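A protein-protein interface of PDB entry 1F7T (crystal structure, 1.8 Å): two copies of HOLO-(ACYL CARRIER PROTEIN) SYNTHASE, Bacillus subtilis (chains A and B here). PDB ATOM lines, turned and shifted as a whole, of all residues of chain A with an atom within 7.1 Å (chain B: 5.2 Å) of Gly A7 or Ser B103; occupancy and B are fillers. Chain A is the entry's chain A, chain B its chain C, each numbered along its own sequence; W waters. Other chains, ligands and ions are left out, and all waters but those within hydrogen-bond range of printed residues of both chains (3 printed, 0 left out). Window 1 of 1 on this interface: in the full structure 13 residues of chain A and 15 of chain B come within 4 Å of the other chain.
Water W2 bridges the side-chain amide oxygen (OE1) of Gln B114 (2.6 Å) and the backbone carbonyl oxygen (O) of Val A115 (3.0 Å). Water W3 lies within hydrogen-bond range of the backbone NH of Ile A6 (3.1 Å), the side-chain amino group of Lys B87 (3.3 Å) and the backbone carbonyl oxygen of Val B102 (3.3 Å). Water W1 bridges NZ of Lys A63 and OG1 of Thr B105.
Gln A114 touches its own counterpart, Gln B114. Positions printed for both chains: 101, 113 and 114.
Hydrophobic or aromatic side chains of chain A that line the printed part of chain B: Ile A6 and Leu A8. Along chain A the printed residues that touch a printed residue of chain B span positions 6 to 114. Among the printed residues, no Asp or Glu carboxylate lies within 4 Å of a Lys or Arg side-chain nitrogen of the other chain.
O of Gly A7 lies within hydrogen-bond range of N of Val A115, at 2.8 Å. The backbone carbonyl oxygen of Leu A8 sits at hydrogen-bond distance from the side-chain amino group of Lys A63. O of Asp A9 is in hydrogen-bond range of N of Ala A113, at 3.0 Å. The side-chain amino group (NZ) of Lys B87 lies within hydrogen-bond range of the backbone carbonyl oxygen (O) of Val B102, at 3.1 Å. The backbone carbonyl oxygen (O) of Ser B103 is in hydrogen-bond range of the backbone NH (N) of Gln B114 (3.1 Å). The backbone NH (N) of Thr B105 sits at hydrogen-bond distance from the backbone carbonyl oxygen (O) of Ala B112 (2.9 Å).
The backbone carbonyl oxygen of Ile A6 sits at hydrogen-bond distance from the side-chain amino group of Lys B87 (2.9 Å). The side-chain amide oxygen (OE1) of Gln B114 sits close to the backbone carbonyl oxygen (O) of Gly A7 (3.1 Å). The backbone NH of Leu A8 is in hydrogen-bond range of the side-chain hydroxyl of Ser B103 (2.9 Å). The side-chain amino group (NZ) of Lys B87 sits at hydrogen-bond distance from the backbone carbonyl oxygen (O) of Lys A63, 3.0 Å away. The backbone carbonyl oxygen of Ile B104 lies within hydrogen-bond range of the side-chain amino group of Lys A63 (3.0 Å). OG1 of Thr B105 sits close to NZ of Lys A63. The side-chain amide nitrogen (NE2) of Gln A114 lies close to the side-chain amide nitrogen (NE2) of Gln B114, at 2.9 Å.
His B101 touches Ile A6 (O to CD1, 3.5 Å). CG1 of Ile A6 touches C of Val B102 (3.95 Å). Ser B103 touches Ile A6 (CB to O, 3.6 Å). Ile A6 touches Gln B114 (CD1 to CG, 3.6 Å). Gly A7 touches Ser B103 (CA to OG, 3.3 Å). Leu A8 touches Thr B105. Ala B113 touches Leu A8 (C to CD2, 3.8 Å). Leu A8 touches Gln B114. Thr B105 touches Asp A9. Lys A63 touches Ser B103.
Gly A7 touches just these residues of chain B: Ser B103 (3.3 Å) and Gln B114 (3.1 Å). Of chain A, only Ile A6, Gly A7, Leu A8 and Lys A63 come within 4 Å of Ser B103. Printed residues of chain B within 4 Å of Gln A114: Gln B114. Printed residues of chain B within 4 Å of Asp A9: Thr B105. Of the printed residues of chain A, Gln B114 touches Ile A6, Gly A7, Leu A8 and Gln A114. Ala A113 touches none of the printed residues of chain B. The nearest residue of chain A that does not touch Ser B103 is Asp A9 (5.6 Å).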
ATOM      1  N   GLY A   5     -12.924  20.819  12.903  1.00  0.00           N
ATOM      2  CA  GLY A   5     -12.678  22.137  12.345  1.00  0.00           C
ATOM      3  C   GLY A   5     -13.941  22.972  12.350  1.00  0.00           C
ATOM      4  O   GLY A   5     -15.036  22.444  12.532  1.00  0.00           O
ATOM      5  N   ILE A   6     -13.790  24.283  12.187  1.00  0.00           N
ATOM      6  CA  ILE A   6     -14.949  25.162  12.142  1.00  0.00           C
ATOM      7  C   ILE A   6     -14.762  26.102  10.956  1.00  0.00           C
ATOM      8  O   ILE A   6     -13.637  26.296  10.481  1.00  0.00           O
ATOM      9  CB  ILE A   6     -15.108  25.988  13.441  1.00  0.00           C
ATOM     10  CG1 ILE A   6     -13.982  27.025  13.574  1.00  0.00           C
ATOM     11  CG2 ILE A   6     -15.106  25.035  14.650  1.00  0.00           C
ATOM     12  CD1 ILE A   6     -14.177  27.955  14.789  1.00  0.00           C
ATOM     13  N   GLY A   7     -15.864  26.667  10.476  1.00  0.00           N
ATOM     14  CA  GLY A   7     -15.780  27.561   9.338  1.00  0.00           C
ATOM     15  C   GLY A   7     -16.842  28.633   9.407  1.00  0.00           C
ATOM     16  O   GLY A   7     -17.960  28.395   9.861  1.00  0.00           O
ATOM     17  N   LEU A   8     -16.484  29.817   8.936  1.00  0.00           N
ATOM     18  CA  LEU A   8     -17.377  30.960   8.945  1.00  0.00           C
ATOM     19  C   LEU A   8     -17.238  31.679   7.613  1.00  0.00           C
ATOM     20  O   LEU A   8     -16.145  31.765   7.069  1.00  0.00           O
ATOM     21  CB  LEU A   8     -16.964  31.908  10.081  1.00  0.00           C
ATOM     22  CG  LEU A   8     -17.683  33.255  10.137  1.00  0.00           C
ATOM     23  CD1 LEU A   8     -19.144  33.043  10.602  1.00  0.00           C
ATOM     24  CD2 LEU A   8     -16.933  34.170  11.106  1.00  0.00           C
ATOM     25  N   ASP A   9     -18.345  32.178   7.077  1.00  0.00           N
ATOM     26  CA  ASP A   9     -18.295  32.925   5.834  1.00  0.00           C
ATOM     27  C   ASP A   9     -19.388  33.983   5.802  1.00  0.00           C
ATOM     28  O   ASP A   9     -20.490  33.763   6.290  1.00  0.00           O
ATOM     29  CB  ASP A   9     -18.478  31.995   4.616  1.00  0.00           C
ATOM     30  CG  ASP A   9     -18.525  32.771   3.304  1.00  0.00           C
ATOM     31  OD1 ASP A   9     -19.621  33.188   2.883  1.00  0.00           O
ATOM     32  OD2 ASP A   9     -17.456  32.994   2.716  1.00  0.00           O
ATOM     33  N   ALA A  56     -22.445  30.711   0.852  1.00  0.00           N
ATOM     34  CA  ALA A  56     -21.860  30.936   2.179  1.00  0.00           C
ATOM     35  C   ALA A  56     -21.724  29.646   2.985  1.00  0.00           C
ATOM     36  O   ALA A  56     -20.711  29.421   3.647  1.00  0.00           O
ATOM     37  CB  ALA A  56     -22.701  31.938   2.949  1.00  0.00           C
ATOM     38  N   ALA A  57     -22.757  28.809   2.948  1.00  0.00           N
ATOM     39  CA  ALA A  57     -22.749  27.554   3.689  1.00  0.00           C
ATOM     40  C   ALA A  57     -21.664  26.619   3.172  1.00  0.00           C
ATOM     41  O   ALA A  57     -20.955  25.987   3.955  1.00  0.00           O
ATOM     42  CB  ALA A  57     -24.126  26.874   3.595  1.00  0.00           C
ATOM     43  N   GLU A  59     -18.956  27.524   1.470  1.00  0.00           N
ATOM     44  CA  GLU A  59     -17.649  28.125   1.740  1.00  0.00           C
ATOM     45  C   GLU A  59     -17.280  27.838   3.205  1.00  0.00           C
ATOM     46  O   GLU A  59     -16.149  27.452   3.497  1.00  0.00           O
ATOM     47  CB  GLU A  59     -17.685  29.643   1.522  1.00  0.00           C
ATOM     48  CG  GLU A  59     -17.616  30.103   0.059  1.00  0.00           C
ATOM     49  CD  GLU A  59     -16.329  29.671  -0.633  1.00  0.00           C
ATOM     50  OE1 GLU A  59     -15.297  29.542   0.061  1.00  0.00           O
ATOM     51  OE2 GLU A  59     -16.341  29.473  -1.870  1.00  0.00           O
ATOM     52  N   ALA A  60     -18.237  28.020   4.116  1.00  0.00           N
ATOM     53  CA  ALA A  60     -17.975  27.757   5.542  1.00  0.00           C
ATOM     54  C   ALA A  60     -17.629  26.277   5.733  1.00  0.00           C
ATOM     55  O   ALA A  60     -16.713  25.912   6.487  1.00  0.00           O
ATOM     56  CB  ALA A  60     -19.205  28.128   6.394  1.00  0.00           C
ATOM     57  N   PHE A  61     -18.358  25.407   5.053  1.00  0.00           N
ATOM     58  CA  PHE A  61     -18.070  23.983   5.191  1.00  0.00           C
ATOM     59  C   PHE A  61     -16.653  23.682   4.711  1.00  0.00           C
ATOM     60  O   PHE A  61     -15.921  22.919   5.345  1.00  0.00           O
ATOM     61  CB  PHE A  61     -19.056  23.136   4.381  1.00  0.00           C
ATOM     62  CG  PHE A  61     -18.764  21.661   4.452  1.00  0.00           C
ATOM     63  CD1 PHE A  61     -19.267  20.891   5.491  1.00  0.00           C
ATOM     64  CD2 PHE A  61     -17.902  21.068   3.531  1.00  0.00           C
ATOM     65  CE1 PHE A  61     -18.909  19.539   5.624  1.00  0.00           C
ATOM     66  CE2 PHE A  61     -17.531  19.716   3.648  1.00  0.00           C
ATOM     67  CZ  PHE A  61     -18.038  18.956   4.700  1.00  0.00           C
ATOM     68  N   SER A  62     -16.261  24.277   3.586  1.00  0.00           N
ATOM     69  CA  SER A  62     -14.930  24.031   3.043  1.00  0.00           C
ATOM     70  C   SER A  62     -13.822  24.523   3.972  1.00  0.00           C
ATOM     71  O   SER A  62     -12.712  23.982   3.970  1.00  0.00           O
ATOM     72  CB  SER A  62     -14.773  24.679   1.662  1.00  0.00           C
ATOM     73  OG  SER A  62     -14.718  26.092   1.755  1.00  0.00           O
ATOM     74  N   LYS A  63     -14.121  25.543   4.765  1.00  0.00           N
ATOM     75  CA  LYS A  63     -13.137  26.076   5.708  1.00  0.00           C
ATOM     76  C   LYS A  63     -13.028  25.140   6.911  1.00  0.00           C
ATOM     77  O   LYS A  63     -11.931  24.877   7.411  1.00  0.00           O
ATOM     78  CB  LYS A  63     -13.540  27.482   6.154  1.00  0.00           C
ATOM     79  CG  LYS A  63     -13.432  28.523   5.032  1.00  0.00           C
ATOM     80  CD  LYS A  63     -13.907  29.892   5.488  1.00  0.00           C
ATOM     81  CE  LYS A  63     -13.583  30.942   4.440  1.00  0.00           C
ATOM     82  NZ  LYS A  63     -13.891  32.318   4.892  1.00  0.00           N
ATOM     83  N   ALA A  64     -14.167  24.632   7.368  1.00  0.00           N
ATOM     84  CA  ALA A  64     -14.177  23.700   8.492  1.00  0.00           C
ATOM     85  C   ALA A  64     -13.462  22.413   8.066  1.00  0.00           C
ATOM     86  O   ALA A  64     -12.769  21.774   8.868  1.00  0.00           O
ATOM     87  CB  ALA A  64     -15.615  23.396   8.909  1.00  0.00           C
ATOM     88  N   PHE A  65     -13.631  22.050   6.796  1.00  0.00           N
ATOM     89  CA  PHE A  65     -13.013  20.856   6.229  1.00  0.00           C
ATOM     90  C   PHE A  65     -11.496  21.057   6.175  1.00  0.00           C
ATOM     91  O   PHE A  65     -10.742  20.089   6.087  1.00  0.00           O
ATOM     92  CB  PHE A  65     -13.575  20.609   4.822  1.00  0.00           C
ATOM     93  CG  PHE A  65     -13.287  19.239   4.280  1.00  0.00           C
ATOM     94  CD1 PHE A  65     -13.921  18.119   4.811  1.00  0.00           C
ATOM     95  CD2 PHE A  65     -12.395  19.070   3.229  1.00  0.00           C
ATOM     96  CE1 PHE A  65     -13.671  16.846   4.297  1.00  0.00           C
ATOM     97  CE2 PHE A  65     -12.138  17.805   2.707  1.00  0.00           C
ATOM     98  CZ  PHE A  65     -12.775  16.694   3.240  1.00  0.00           C
ATOM     99  N   HIS A 101     -22.547  20.218  11.495  1.00  0.00           N
ATOM    100  CA  HIS A 101     -23.546  21.165  11.990  1.00  0.00           C
ATOM    101  C   HIS A 101     -23.372  22.456  11.196  1.00  0.00           C
ATOM    102  O   HIS A 101     -22.244  22.877  10.928  1.00  0.00           O
ATOM    103  CB  HIS A 101     -23.328  21.452  13.475  1.00  0.00           C
ATOM    104  CG  HIS A 101     -23.383  20.225  14.327  1.00  0.00           C
ATOM    105  ND1 HIS A 101     -24.571  19.658  14.732  1.00  0.00           N
ATOM    106  CD2 HIS A 101     -22.401  19.402  14.762  1.00  0.00           C
ATOM    107  CE1 HIS A 101     -24.318  18.533  15.377  1.00  0.00           C
ATOM    108  NE2 HIS A 101     -23.009  18.354  15.408  1.00  0.00           N
ATOM    109  N   ALA A 113     -22.848  32.105   7.046  1.00  0.00           N
ATOM    110  CA  ALA A 113     -23.047  30.751   7.522  1.00  0.00           C
ATOM    111  C   ALA A 113     -21.848  30.282   8.321  1.00  0.00           C
ATOM    112  O   ALA A 113     -20.755  30.810   8.183  1.00  0.00           O
ATOM    113  CB  ALA A 113     -23.300  29.798   6.327  1.00  0.00           C
ATOM    114  N   GLN A 114     -22.059  29.300   9.185  1.00  0.00           N
ATOM    115  CA  GLN A 114     -20.954  28.756   9.957  1.00  0.00           C
ATOM    116  C   GLN A 114     -21.158  27.263   9.979  1.00  0.00           C
ATOM    117  O   GLN A 114     -22.284  26.774   9.914  1.00  0.00           O
ATOM    118  CB  GLN A 114     -20.943  29.280  11.399  1.00  0.00           C
ATOM    119  CG  GLN A 114     -22.150  28.873  12.209  1.00  0.00           C
ATOM    120  CD  GLN A 114     -22.105  29.377  13.637  1.00  0.00           C
ATOM    121  OE1 GLN A 114     -22.955  29.025  14.453  1.00  0.00           O
ATOM    122  NE2 GLN A 114     -21.122  30.217  13.942  1.00  0.00           N
ATOM    123  N   VAL A 115     -20.059  26.544  10.091  1.00  0.00           N
ATOM    124  CA  VAL A 115     -20.127  25.101  10.127  1.00  0.00           C
ATOM    125  C   VAL A 115     -19.179  24.600  11.196  1.00  0.00           C
ATOM    126  O   VAL A 115     -18.124  25.203  11.447  1.00  0.00           O
ATOM    127  CB  VAL A 115     -19.684  24.499   8.759  1.00  0.00           C
ATOM    128  CG1 VAL A 115     -19.356  22.989   8.914  1.00  0.00           C
ATOM    129  CG2 VAL A 115     -20.778  24.714   7.716  1.00  0.00           C
ATOM    130  N   VAL A 116     -19.573  23.519  11.852  1.00  0.00           N
ATOM    131  CA  VAL A 116     -18.693  22.869  12.809  1.00  0.00           C
ATOM    132  C   VAL A 116     -18.684  21.398  12.413  1.00  0.00           C
ATOM    133  O   VAL A 116     -19.745  20.805  12.194  1.00  0.00           O
ATOM    134  CB  VAL A 116     -19.185  22.974  14.267  1.00  0.00           C
ATOM    135  CG1 VAL A 116     -18.263  22.147  15.173  1.00  0.00           C
ATOM    136  CG2 VAL A 116     -19.195  24.424  14.716  1.00  0.00           C
ATOM    137  N   ILE A 117     -17.489  20.832  12.262  1.00  0.00           N
ATOM    138  CA  ILE A 117     -17.351  19.413  11.942  1.00  0.00           C
ATOM    139  C   ILE A 117     -16.728  18.762  13.176  1.00  0.00           C
ATOM    140  O   ILE A 117     -15.744  19.270  13.714  1.00  0.00           O
ATOM    141  CB  ILE A 117     -16.421  19.182  10.743  1.00  0.00           C
ATOM    142  CG1 ILE A 117     -17.042  19.803   9.485  1.00  0.00           C
ATOM    143  CG2 ILE A 117     -16.180  17.674  10.553  1.00  0.00           C
ATOM    144  CD1 ILE A 117     -16.152  19.753   8.261  1.00  0.00           C
ATOM    145  N   LYS B  87      -5.040  26.998   5.788  1.00  0.00           N
ATOM    146  CA  LYS B  87      -5.999  27.097   6.884  1.00  0.00           C
ATOM    147  C   LYS B  87      -5.387  27.827   8.084  1.00  0.00           C
ATOM    148  O   LYS B  87      -4.308  27.468   8.545  1.00  0.00           O
ATOM    149  CB  LYS B  87      -6.435  25.698   7.326  1.00  0.00           C
ATOM    150  CG  LYS B  87      -7.276  25.671   8.610  1.00  0.00           C
ATOM    151  CD  LYS B  87      -8.667  26.260   8.408  1.00  0.00           C
ATOM    152  CE  LYS B  87      -9.423  26.311   9.742  1.00  0.00           C
ATOM    153  NZ  LYS B  87     -10.876  26.629   9.543  1.00  0.00           N
ATOM    154  N   PRO B  88      -6.068  28.858   8.603  1.00  0.00           N
ATOM    155  CA  PRO B  88      -5.491  29.555   9.757  1.00  0.00           C
ATOM    156  C   PRO B  88      -5.659  28.763  11.038  1.00  0.00           C
ATOM    157  O   PRO B  88      -6.649  28.053  11.212  1.00  0.00           O
ATOM    158  CB  PRO B  88      -6.277  30.860   9.813  1.00  0.00           C
ATOM    159  CG  PRO B  88      -7.627  30.457   9.295  1.00  0.00           C
ATOM    160  CD  PRO B  88      -7.263  29.563   8.107  1.00  0.00           C
ATOM    161  N   HIS B 101      -9.653  26.190  17.638  1.00  0.00           N
ATOM    162  CA  HIS B 101     -10.090  26.159  16.249  1.00  0.00           C
ATOM    163  C   HIS B 101     -10.545  27.568  15.892  1.00  0.00           C
ATOM    164  O   HIS B 101     -11.250  28.197  16.680  1.00  0.00           O
ATOM    165  CB  HIS B 101     -11.245  25.173  16.099  1.00  0.00           C
ATOM    166  CG  HIS B 101     -10.882  23.775  16.499  1.00  0.00           C
ATOM    167  ND1 HIS B 101     -10.193  22.923  15.667  1.00  0.00           N
ATOM    168  CD2 HIS B 101     -11.061  23.106  17.663  1.00  0.00           C
ATOM    169  CE1 HIS B 101      -9.964  21.784  16.300  1.00  0.00           C
ATOM    170  NE2 HIS B 101     -10.480  21.872  17.513  1.00  0.00           N
ATOM    171  N   VAL B 102     -10.138  28.056  14.718  1.00  0.00           N
ATOM    172  CA  VAL B 102     -10.510  29.406  14.271  1.00  0.00           C
ATOM    173  C   VAL B 102     -10.910  29.388  12.795  1.00  0.00           C
ATOM    174  O   VAL B 102     -10.558  28.466  12.065  1.00  0.00           O
ATOM    175  CB  VAL B 102      -9.310  30.405  14.442  1.00  0.00           C
ATOM    176  CG1 VAL B 102      -8.134  29.966  13.568  1.00  0.00           C
ATOM    177  CG2 VAL B 102      -9.727  31.846  14.082  1.00  0.00           C
ATOM    178  N   SER B 103     -11.673  30.394  12.378  1.00  0.00           N
ATOM    179  CA  SER B 103     -12.034  30.550  10.967  1.00  0.00           C
ATOM    180  C   SER B 103     -12.124  32.052  10.748  1.00  0.00           C
ATOM    181  O   SER B 103     -12.598  32.787  11.614  1.00  0.00           O
ATOM    182  CB  SER B 103     -13.364  29.884  10.611  1.00  0.00           C
ATOM    183  OG  SER B 103     -13.596  30.042   9.209  1.00  0.00           O
ATOM    184  N   ILE B 104     -11.630  32.513   9.605  1.00  0.00           N
ATOM    185  CA  ILE B 104     -11.626  33.936   9.301  1.00  0.00           C
ATOM    186  C   ILE B 104     -12.274  34.138   7.936  1.00  0.00           C
ATOM    187  O   ILE B 104     -12.076  33.331   7.030  1.00  0.00           O
ATOM    188  CB  ILE B 104     -10.170  34.478   9.248  1.00  0.00           C
ATOM    189  CG1 ILE B 104      -9.464  34.220  10.586  1.00  0.00           C
ATOM    190  CG2 ILE B 104     -10.177  35.987   8.954  1.00  0.00           C
ATOM    191  CD1 ILE B 104      -7.984  34.624  10.598  1.00  0.00           C
ATOM    192  N   THR B 105     -13.051  35.208   7.795  1.00  0.00           N
ATOM    193  CA  THR B 105     -13.713  35.514   6.526  1.00  0.00           C
ATOM    194  C   THR B 105     -13.664  37.026   6.250  1.00  0.00           C
ATOM    195  O   THR B 105     -13.396  37.818   7.149  1.00  0.00           O
ATOM    196  CB  THR B 105     -15.190  35.000   6.525  1.00  0.00           C
ATOM    197  OG1 THR B 105     -15.760  35.182   5.228  1.00  0.00           O
ATOM    198  CG2 THR B 105     -16.036  35.749   7.541  1.00  0.00           C
ATOM    199  N   ALA B 112     -14.281  39.131   9.643  1.00  0.00           N
ATOM    200  CA  ALA B 112     -14.983  38.488  10.747  1.00  0.00           C
ATOM    201  C   ALA B 112     -14.260  37.195  11.099  1.00  0.00           C
ATOM    202  O   ALA B 112     -13.562  36.625  10.265  1.00  0.00           O
ATOM    203  CB  ALA B 112     -16.444  38.202  10.360  1.00  0.00           C
ATOM    204  N   ALA B 113     -14.408  36.753  12.341  1.00  0.00           N
ATOM    205  CA  ALA B 113     -13.750  35.529  12.768  1.00  0.00           C
ATOM    206  C   ALA B 113     -14.501  34.878  13.910  1.00  0.00           C
ATOM    207  O   ALA B 113     -15.255  35.533  14.626  1.00  0.00           O
ATOM    208  CB  ALA B 113     -12.325  35.831  13.205  1.00  0.00           C
ATOM    209  N   GLN B 114     -14.292  33.578  14.082  1.00  0.00           N
ATOM    210  CA  GLN B 114     -14.930  32.871  15.186  1.00  0.00           C
ATOM    211  C   GLN B 114     -13.889  31.902  15.726  1.00  0.00           C
ATOM    212  O   GLN B 114     -12.979  31.495  15.011  1.00  0.00           O
ATOM    213  CB  GLN B 114     -16.181  32.114  14.722  1.00  0.00           C
ATOM    214  CG  GLN B 114     -15.904  30.969  13.772  1.00  0.00           C
ATOM    215  CD  GLN B 114     -17.165  30.210  13.353  1.00  0.00           C
ATOM    216  OE1 GLN B 114     -17.080  29.139  12.765  1.00  0.00           O
ATOM    217  NE2 GLN B 114     -18.332  30.772  13.649  1.00  0.00           N
HETATM  218  O   HOH W   1     -13.543  34.786   2.954  1.00  0.00           O
HETATM  219  O   HOH W   2     -18.752  27.350  13.508  1.00  0.00           O
HETATM  220  O   HOH W   3     -10.879  25.242  12.483  1.00  0.00           O
